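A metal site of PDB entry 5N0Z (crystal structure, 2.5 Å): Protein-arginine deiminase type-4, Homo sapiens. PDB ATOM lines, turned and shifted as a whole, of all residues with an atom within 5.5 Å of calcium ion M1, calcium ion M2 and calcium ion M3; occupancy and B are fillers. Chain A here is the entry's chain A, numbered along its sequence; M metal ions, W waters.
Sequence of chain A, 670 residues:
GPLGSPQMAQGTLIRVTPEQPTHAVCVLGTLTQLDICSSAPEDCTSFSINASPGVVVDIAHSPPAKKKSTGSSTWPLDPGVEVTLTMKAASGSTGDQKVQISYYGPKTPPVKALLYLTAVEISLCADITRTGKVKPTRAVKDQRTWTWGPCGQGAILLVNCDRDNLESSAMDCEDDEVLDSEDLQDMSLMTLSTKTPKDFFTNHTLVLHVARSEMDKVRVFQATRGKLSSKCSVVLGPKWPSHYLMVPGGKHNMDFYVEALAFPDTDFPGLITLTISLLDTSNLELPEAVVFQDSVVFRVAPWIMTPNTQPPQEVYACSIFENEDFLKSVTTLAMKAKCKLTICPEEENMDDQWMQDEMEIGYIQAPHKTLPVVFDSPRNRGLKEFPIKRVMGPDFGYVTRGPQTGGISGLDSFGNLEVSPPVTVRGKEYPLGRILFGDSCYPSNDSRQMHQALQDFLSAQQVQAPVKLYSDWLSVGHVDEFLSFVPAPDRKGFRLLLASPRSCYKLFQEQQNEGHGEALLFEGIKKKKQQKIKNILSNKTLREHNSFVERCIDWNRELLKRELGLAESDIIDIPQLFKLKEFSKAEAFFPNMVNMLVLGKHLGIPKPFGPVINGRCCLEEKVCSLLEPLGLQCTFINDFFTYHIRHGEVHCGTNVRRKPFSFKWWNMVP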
ATOM      1  N   ASN A 160      -0.622 -11.733   6.152  1.00  0.00           N
ATOM      2  CA  ASN A 160      -0.482 -11.173   4.821  1.00  0.00           C
ATOM      3  C   ASN A 160      -0.498 -12.295   3.780  1.00  0.00           C
ATOM      4  O   ASN A 160       0.470 -12.564   3.106  1.00  0.00           O
ATOM      5  CB  ASN A 160       0.798 -10.327   4.767  1.00  0.00           C
ATOM      6  CG  ASN A 160       0.875  -9.458   3.548  1.00  0.00           C
ATOM      7  OD1 ASN A 160      -0.142  -8.975   3.064  1.00  0.00           O
ATOM      8  ND2 ASN A 160       2.090  -9.238   3.060  1.00  0.00           N
ATOM      9  N   ASP A 162      -2.731 -12.757   1.162  1.00  0.00           N
ATOM     10  CA  ASP A 162      -3.184 -12.457  -0.214  1.00  0.00           C
ATOM     11  C   ASP A 162      -2.003 -12.356  -1.197  1.00  0.00           C
ATOM     12  O   ASP A 162      -0.831 -12.460  -0.815  1.00  0.00           O
ATOM     13  CB  ASP A 162      -4.125 -11.212  -0.267  1.00  0.00           C
ATOM     14  CG  ASP A 162      -3.404  -9.889  -0.001  1.00  0.00           C
ATOM     15  OD1 ASP A 162      -2.173  -9.919   0.245  1.00  0.00           O
ATOM     16  OD2 ASP A 162      -4.059  -8.804   0.005  1.00  0.00           O
ATOM     17  N   ARG A 163      -2.354 -12.154  -2.464  1.00  0.00           N
ATOM     18  CA  ARG A 163      -1.397 -11.957  -3.571  1.00  0.00           C
ATOM     19  C   ARG A 163      -1.718 -10.618  -4.205  1.00  0.00           C
ATOM     20  O   ARG A 163      -2.598 -10.512  -5.073  1.00  0.00           O
ATOM     21  CB  ARG A 163      -1.573 -13.100  -4.558  1.00  0.00           C
ATOM     22  CG  ARG A 163      -0.469 -13.311  -5.564  1.00  0.00           C
ATOM     23  CD  ARG A 163      -0.597 -14.726  -6.104  1.00  0.00           C
ATOM     24  NE  ARG A 163      -1.830 -14.965  -6.854  1.00  0.00           N
ATOM     25  CZ  ARG A 163      -2.333 -16.167  -7.197  1.00  0.00           C
ATOM     26  NH1 ARG A 163      -1.715 -17.314  -6.872  1.00  0.00           N
ATOM     27  NH2 ARG A 163      -3.473 -16.231  -7.860  1.00  0.00           N
ATOM     28  N   ASP A 164      -1.062  -9.570  -3.699  1.00  0.00           N
ATOM     29  CA  ASP A 164      -1.083  -8.228  -4.303  1.00  0.00           C
ATOM     30  C   ASP A 164      -0.086  -8.188  -5.454  1.00  0.00           C
ATOM     31  O   ASP A 164      -0.309  -7.519  -6.477  1.00  0.00           O
ATOM     32  CB  ASP A 164      -0.733  -7.139  -3.281  1.00  0.00           C
ATOM     33  CG  ASP A 164      -1.897  -6.758  -2.414  1.00  0.00           C
ATOM     34  OD1 ASP A 164      -3.037  -6.742  -2.883  1.00  0.00           O
ATOM     35  OD2 ASP A 164      -1.677  -6.426  -1.236  1.00  0.00           O
ATOM     36  N   ASP A 172       2.054 -13.051  -0.447  1.00  0.00           N
ATOM     37  CA  ASP A 172       2.989 -11.953  -0.196  1.00  0.00           C
ATOM     38  C   ASP A 172       4.037 -12.229   0.881  1.00  0.00           C
ATOM     39  O   ASP A 172       5.205 -11.870   0.702  1.00  0.00           O
ATOM     40  CB  ASP A 172       2.213 -10.697   0.222  1.00  0.00           C
ATOM     41  CG  ASP A 172       1.352 -10.151  -0.872  1.00  0.00           C
ATOM     42  OD1 ASP A 172       1.498 -10.580  -2.043  1.00  0.00           O
ATOM     43  OD2 ASP A 172       0.509  -9.287  -0.575  1.00  0.00           O
ATOM     44  N   CYS A 173       3.606 -12.850   1.974  1.00  0.00           N
ATOM     45  CA  CYS A 173       4.398 -13.022   3.194  1.00  0.00           C
ATOM     46  C   CYS A 173       5.391 -14.202   3.183  1.00  0.00           C
ATOM     47  O   CYS A 173       6.162 -14.371   4.143  1.00  0.00           O
ATOM     48  CB  CYS A 173       3.454 -13.106   4.406  1.00  0.00           C
ATOM     49  SG  CYS A 173       2.341 -14.553   4.495  1.00  0.00           S
ATOM     50  N   GLU A 174       5.392 -15.020   2.116  1.00  0.00           N
ATOM     51  CA  GLU A 174       6.335 -16.161   2.052  1.00  0.00           C
ATOM     52  C   GLU A 174       7.795 -15.772   1.786  1.00  0.00           C
ATOM     53  O   GLU A 174       8.690 -16.541   2.110  1.00  0.00           O
ATOM     54  CB  GLU A 174       5.842 -17.246   1.076  1.00  0.00           C
ATOM     55  CG  GLU A 174       4.982 -18.313   1.734  1.00  0.00           C
ATOM     56  CD  GLU A 174       3.907 -18.917   0.831  1.00  0.00           C
ATOM     57  OE1 GLU A 174       4.052 -18.904  -0.419  1.00  0.00           O
ATOM     58  OE2 GLU A 174       2.912 -19.459   1.372  1.00  0.00           O
ATOM     59  N   ASP A 175       8.057 -14.586   1.234  1.00  0.00           N
ATOM     60  CA  ASP A 175       9.424 -14.155   0.923  1.00  0.00           C
ATOM     61  C   ASP A 175       9.832 -13.068   1.917  1.00  0.00           C
ATOM     62  O   ASP A 175       9.064 -12.758   2.827  1.00  0.00           O
ATOM     63  CB  ASP A 175       9.487 -13.612  -0.517  1.00  0.00           C
ATOM     64  CG  ASP A 175       8.673 -12.307  -0.710  1.00  0.00           C
ATOM     65  OD1 ASP A 175       8.137 -11.735   0.269  1.00  0.00           O
ATOM     66  OD2 ASP A 175       8.541 -11.846  -1.867  1.00  0.00           O
ATOM     67  N   ASP A 176      11.008 -12.469   1.716  1.00  0.00           N
ATOM     68  CA  ASP A 176      11.531 -11.428   2.629  1.00  0.00           C
ATOM     69  C   ASP A 176      11.389  -9.950   2.183  1.00  0.00           C
ATOM     70  O   ASP A 176      11.993  -9.070   2.820  1.00  0.00           O
ATOM     71  CB  ASP A 176      13.016 -11.728   2.926  1.00  0.00           C
ATOM     72  CG  ASP A 176      13.210 -12.903   3.873  1.00  0.00           C
ATOM     73  OD1 ASP A 176      12.408 -13.097   4.820  1.00  0.00           O
ATOM     74  OD2 ASP A 176      14.211 -13.633   3.684  1.00  0.00           O
ATOM     75  N   GLU A 177      10.588  -9.660   1.143  1.00  0.00           N
ATOM     76  CA  GLU A 177      10.526  -8.302   0.518  1.00  0.00           C
ATOM     77  C   GLU A 177       9.112  -7.718   0.368  1.00  0.00           C
ATOM     78  O   GLU A 177       8.146  -8.465   0.151  1.00  0.00           O
ATOM     79  CB  GLU A 177      11.146  -8.319  -0.890  1.00  0.00           C
ATOM     80  CG  GLU A 177      12.270  -9.325  -1.115  1.00  0.00           C
ATOM     81  CD  GLU A 177      12.962  -9.144  -2.462  1.00  0.00           C
ATOM     82  OE1 GLU A 177      13.435  -8.017  -2.753  1.00  0.00           O
ATOM     83  OE2 GLU A 177      13.055 -10.130  -3.208  1.00  0.00           O
ATOM     84  N   VAL A 178       9.005  -6.386   0.456  1.00  0.00           N
ATOM     85  CA  VAL A 178       7.827  -5.618  -0.005  1.00  0.00           C
ATOM     86  C   VAL A 178       8.046  -5.238  -1.474  1.00  0.00           C
ATOM     87  O   VAL A 178       8.896  -4.392  -1.790  1.00  0.00           O
ATOM     88  CB  VAL A 178       7.624  -4.313   0.783  1.00  0.00           C
ATOM     89  CG1 VAL A 178       6.494  -3.488   0.194  1.00  0.00           C
ATOM     90  CG2 VAL A 178       7.345  -4.585   2.241  1.00  0.00           C
ATOM     91  N   LEU A 179       7.259  -5.826  -2.370  1.00  0.00           N
ATOM     92  CA  LEU A 179       7.446  -5.618  -3.806  1.00  0.00           C
ATOM     93  C   LEU A 179       6.512  -4.551  -4.357  1.00  0.00           C
ATOM     94  O   LEU A 179       6.921  -3.757  -5.182  1.00  0.00           O
ATOM     95  CB  LEU A 179       7.289  -6.936  -4.552  1.00  0.00           C
ATOM     96  CG  LEU A 179       8.333  -7.969  -4.147  1.00  0.00           C
ATOM     97  CD1 LEU A 179       7.980  -9.335  -4.713  1.00  0.00           C
ATOM     98  CD2 LEU A 179       9.752  -7.561  -4.556  1.00  0.00           C
ATOM     99  N   GLU A 182       1.193  -1.212  -2.556  1.00  0.00           N
ATOM    100  CA  GLU A 182      -0.145  -1.660  -2.183  1.00  0.00           C
ATOM    101  C   GLU A 182      -0.072  -2.600  -0.989  1.00  0.00           C
ATOM    102  O   GLU A 182      -0.901  -2.532  -0.070  1.00  0.00           O
ATOM    103  CB  GLU A 182      -0.845  -2.418  -3.339  1.00  0.00           C
ATOM    104  CG  GLU A 182      -1.463  -1.561  -4.452  1.00  0.00           C
ATOM    105  CD  GLU A 182      -0.454  -1.043  -5.483  1.00  0.00           C
ATOM    106  OE1 GLU A 182      -0.709   0.061  -5.993  1.00  0.00           O
ATOM    107  OE2 GLU A 182       0.578  -1.716  -5.766  1.00  0.00           O
ATOM    108  N   ASP A 183       0.932  -3.485  -1.040  1.00  0.00           N
ATOM    109  CA  ASP A 183       1.208  -4.473   0.006  1.00  0.00           C
ATOM    110  C   ASP A 183       1.251  -3.846   1.405  1.00  0.00           C
ATOM    111  O   ASP A 183       0.685  -4.406   2.360  1.00  0.00           O
ATOM    112  CB  ASP A 183       2.527  -5.228  -0.312  1.00  0.00           C
ATOM    113  CG  ASP A 183       2.662  -6.550   0.434  1.00  0.00           C
ATOM    114  OD1 ASP A 183       1.625  -7.115   0.821  1.00  0.00           O
ATOM    115  OD2 ASP A 183       3.821  -7.040   0.586  1.00  0.00           O
ATOM    116  N   ASP A 186      -1.812  -3.670   3.754  1.00  0.00           N
ATOM    117  CA  ASP A 186      -2.148  -4.845   4.546  1.00  0.00           C
ATOM    118  C   ASP A 186      -1.409  -4.894   5.884  1.00  0.00           C
ATOM    119  O   ASP A 186      -1.890  -5.501   6.847  1.00  0.00           O
ATOM    120  CB  ASP A 186      -1.887  -6.123   3.721  1.00  0.00           C
ATOM    121  CG  ASP A 186      -2.780  -6.207   2.483  1.00  0.00           C
ATOM    122  OD1 ASP A 186      -3.914  -5.633   2.477  1.00  0.00           O
ATOM    123  OD2 ASP A 186      -2.328  -6.834   1.477  1.00  0.00           O
ATOM    124  N   PHE A 221       9.435  -4.717   8.600  1.00  0.00           N
ATOM    125  CA  PHE A 221      10.213  -3.929   7.643  1.00  0.00           C
ATOM    126  C   PHE A 221      10.464  -2.526   8.142  1.00  0.00           C
ATOM    127  O   PHE A 221       9.566  -1.875   8.696  1.00  0.00           O
ATOM    128  CB  PHE A 221       9.448  -3.827   6.347  1.00  0.00           C
ATOM    129  CG  PHE A 221       9.197  -5.136   5.688  1.00  0.00           C
ATOM    130  CD1 PHE A 221      10.162  -5.718   4.893  1.00  0.00           C
ATOM    131  CD2 PHE A 221       7.966  -5.777   5.843  1.00  0.00           C
ATOM    132  CE1 PHE A 221       9.926  -6.928   4.270  1.00  0.00           C
ATOM    133  CE2 PHE A 221       7.718  -6.990   5.211  1.00  0.00           C
ATOM    134  CZ  PHE A 221       8.694  -7.568   4.425  1.00  0.00           C
ATOM    135  N   GLU A 259       3.873  -7.552   9.227  1.00  0.00           N
ATOM    136  CA  GLU A 259       2.951  -8.537   8.709  1.00  0.00           C
ATOM    137  C   GLU A 259       3.111  -9.773   9.564  1.00  0.00           C
ATOM    138  O   GLU A 259       4.198 -10.081  10.012  1.00  0.00           O
ATOM    139  CB  GLU A 259       3.239  -8.884   7.218  1.00  0.00           C
ATOM    140  CG  GLU A 259       4.724  -9.118   6.908  1.00  0.00           C
ATOM    141  CD  GLU A 259       5.050  -9.654   5.504  1.00  0.00           C
ATOM    142  OE1 GLU A 259       4.371  -9.289   4.509  1.00  0.00           O
ATOM    143  OE2 GLU A 259       6.030 -10.453   5.413  1.00  0.00           O
ATOM    144  N   LYS A 369      -7.587  -2.317   7.619  1.00  0.00           N
ATOM    145  CA  LYS A 369      -7.718  -3.181   6.453  1.00  0.00           C
ATOM    146  C   LYS A 369      -8.615  -4.370   6.753  1.00  0.00           C
ATOM    147  O   LYS A 369      -8.590  -4.920   7.826  1.00  0.00           O
ATOM    148  CB  LYS A 369      -6.357  -3.669   5.965  1.00  0.00           C
ATOM    149  CG  LYS A 369      -6.409  -4.630   4.783  1.00  0.00           C
ATOM    150  CD  LYS A 369      -7.103  -4.066   3.544  1.00  0.00           C
ATOM    151  CE  LYS A 369      -6.279  -3.044   2.793  1.00  0.00           C
ATOM    152  NZ  LYS A 369      -6.762  -2.944   1.397  1.00  0.00           N
ATOM    153  N   LEU A 371     -10.142  -7.806   4.516  1.00  0.00           N
ATOM    154  CA  LEU A 371     -10.097  -8.429   3.250  1.00  0.00           C
ATOM    155  C   LEU A 371     -10.536  -9.875   3.325  1.00  0.00           C
ATOM    156  O   LEU A 371     -10.263 -10.567   4.300  1.00  0.00           O
ATOM    157  CB  LEU A 371      -8.709  -8.273   2.668  1.00  0.00           C
ATOM    158  CG  LEU A 371      -7.554  -8.926   3.401  1.00  0.00           C
ATOM    159  CD1 LEU A 371      -7.291 -10.286   2.777  1.00  0.00           C
ATOM    160  CD2 LEU A 371      -6.258  -8.168   3.329  1.00  0.00           C
ATOM    161  N   PRO A 394      -5.401 -10.077  -5.566  1.00  0.00           N
ATOM    162  CA  PRO A 394      -5.334  -8.728  -5.020  1.00  0.00           C
ATOM    163  C   PRO A 394      -6.452  -8.473  -4.021  1.00  0.00           C
ATOM    164  O   PRO A 394      -7.615  -8.451  -4.415  1.00  0.00           O
ATOM    165  CB  PRO A 394      -5.493  -7.841  -6.264  1.00  0.00           C
ATOM    166  CG  PRO A 394      -4.922  -8.663  -7.373  1.00  0.00           C
ATOM    167  CD  PRO A 394      -5.185 -10.102  -7.032  1.00  0.00           C
ATOM    168  N   ASP A 395      -6.111  -8.302  -2.755  1.00  0.00           N
ATOM    169  CA  ASP A 395      -7.106  -8.166  -1.670  1.00  0.00           C
ATOM    170  C   ASP A 395      -8.013  -9.426  -1.515  1.00  0.00           C
ATOM    171  O   ASP A 395      -9.204  -9.331  -1.175  1.00  0.00           O
ATOM    172  CB  ASP A 395      -7.925  -6.857  -1.822  1.00  0.00           C
ATOM    173  CG  ASP A 395      -7.164  -5.626  -1.377  1.00  0.00           C
ATOM    174  OD1 ASP A 395      -5.937  -5.693  -1.199  1.00  0.00           O
ATOM    175  OD2 ASP A 395      -7.811  -4.587  -1.165  1.00  0.00           O
HETATM  176 CA    CA M   1       6.482  -9.965   0.476  1.00  0.00          CA
HETATM  177 CA    CA M   2      -0.635  -8.142   0.701  1.00  0.00          CA
HETATM  178 CA    CA M   3      -4.037  -6.493  -0.113  1.00  0.00          CA
HETATM  179  O   HOH W   1       7.474 -10.576   2.659  1.00  0.00           O
HETATM  180  O   HOH W   2       6.056 -10.527  -1.917  1.00  0.00           O
HETATM  181  O   HOH W   3       5.315  -8.823   1.699  1.00  0.00           O
HETATM  182  O   HOH W   4      -3.262  -4.274  -0.384  1.00  0.00           O
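Water W1 bridges the backbone carbonyl oxygen (O) of Asp 175 (2.7 Å) and the side-chain carboxylate (OE2) of Glu 259 (3.1 Å). Water W3 lies within hydrogen-bond range of the side-chain carboxylate (OD2) of Asp 183 and the side-chain carboxylate (OE1) of Glu 259.
Six residues have an atom within 4 Å of calcium ion M2: Asn 160, Asp 162, Asp 164, Asp 172, Asp 183 and Asp 186. Along chain A the residues within 4 Å of calcium ion M2 span positions 160 to 186. The nearest printed residue that does not touch calcium ion M2 is Arg 163 (5.4 Å).
Along chain A the residues within 4 Å of calcium ion M1 span positions 172 to 183. The nearest printed residue that does not touch calcium ion M1 is Cys 173 (4.3 Å).
Calcium ion M2 is bound by the side-chain carboxylate of Asp 172 (2.1 Å), the side-chain carboxylate of Asp 186 (2.3 Å), the side-chain carboxylate of Asp 162 (2.4 Å), the side-chain carboxylate of Asp 183 (2.5 Å), the side-chain amide oxygen of Asn 160 (2.6 Å) and the side-chain carboxylate of Asp 164 (2.8 Å). Calcium ion M2 has six donor atoms within binding distance.
The backbone carbonyl oxygen (O) of Asn 160 is in hydrogen-bond range of the side-chain sulfur (SG) of Cys 173, 3.1 Å away. OD2 of Asp 395 lies within salt-bridge range of NZ of Lys 369, 3.2 Å away. The side-chain carboxylate (OE1) of Glu 259 sits at hydrogen-bond distance from the side-chain amide nitrogen (ND2) of Asn 160 (2.7 Å).
Calcium ion M1 is bound by water W3 (2.0 Å), O of Glu 177 (2.3 Å), O of Asp 172 (2.3 Å), OD1 of Asp 175 (2.4 Å), water W1 (2.5 Å) and water W2 (2.5 Å). Calcium ion M1 has six donor atoms within binding distance.
Of the 21 residues printed, 4 come within 4 Å of calcium ion M3. Along chain A the residues within 4 Å of calcium ion M3 span positions 162 to 395. The nearest printed residue that does not touch calcium ion M3 is Leu 371 (4.4 Å).
Calcium ion M3 is bound by the side-chain carboxylate (OD2) of Asp 162 (2.3 Å), the side-chain carboxylate (OD1) of Asp 395 (2.3 Å), the side-chain carboxylate (OD2) of Asp 186 (2.4 Å), water W4 (2.4 Å), the side-chain carboxylate (OD2) of Asp 164 (2.6 Å) and the side-chain carboxylate (OD1) of Asp 186 (2.7 Å). Slightly farther from calcium ion M3 lies OD1 of Asp 164 (3.0 Å).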
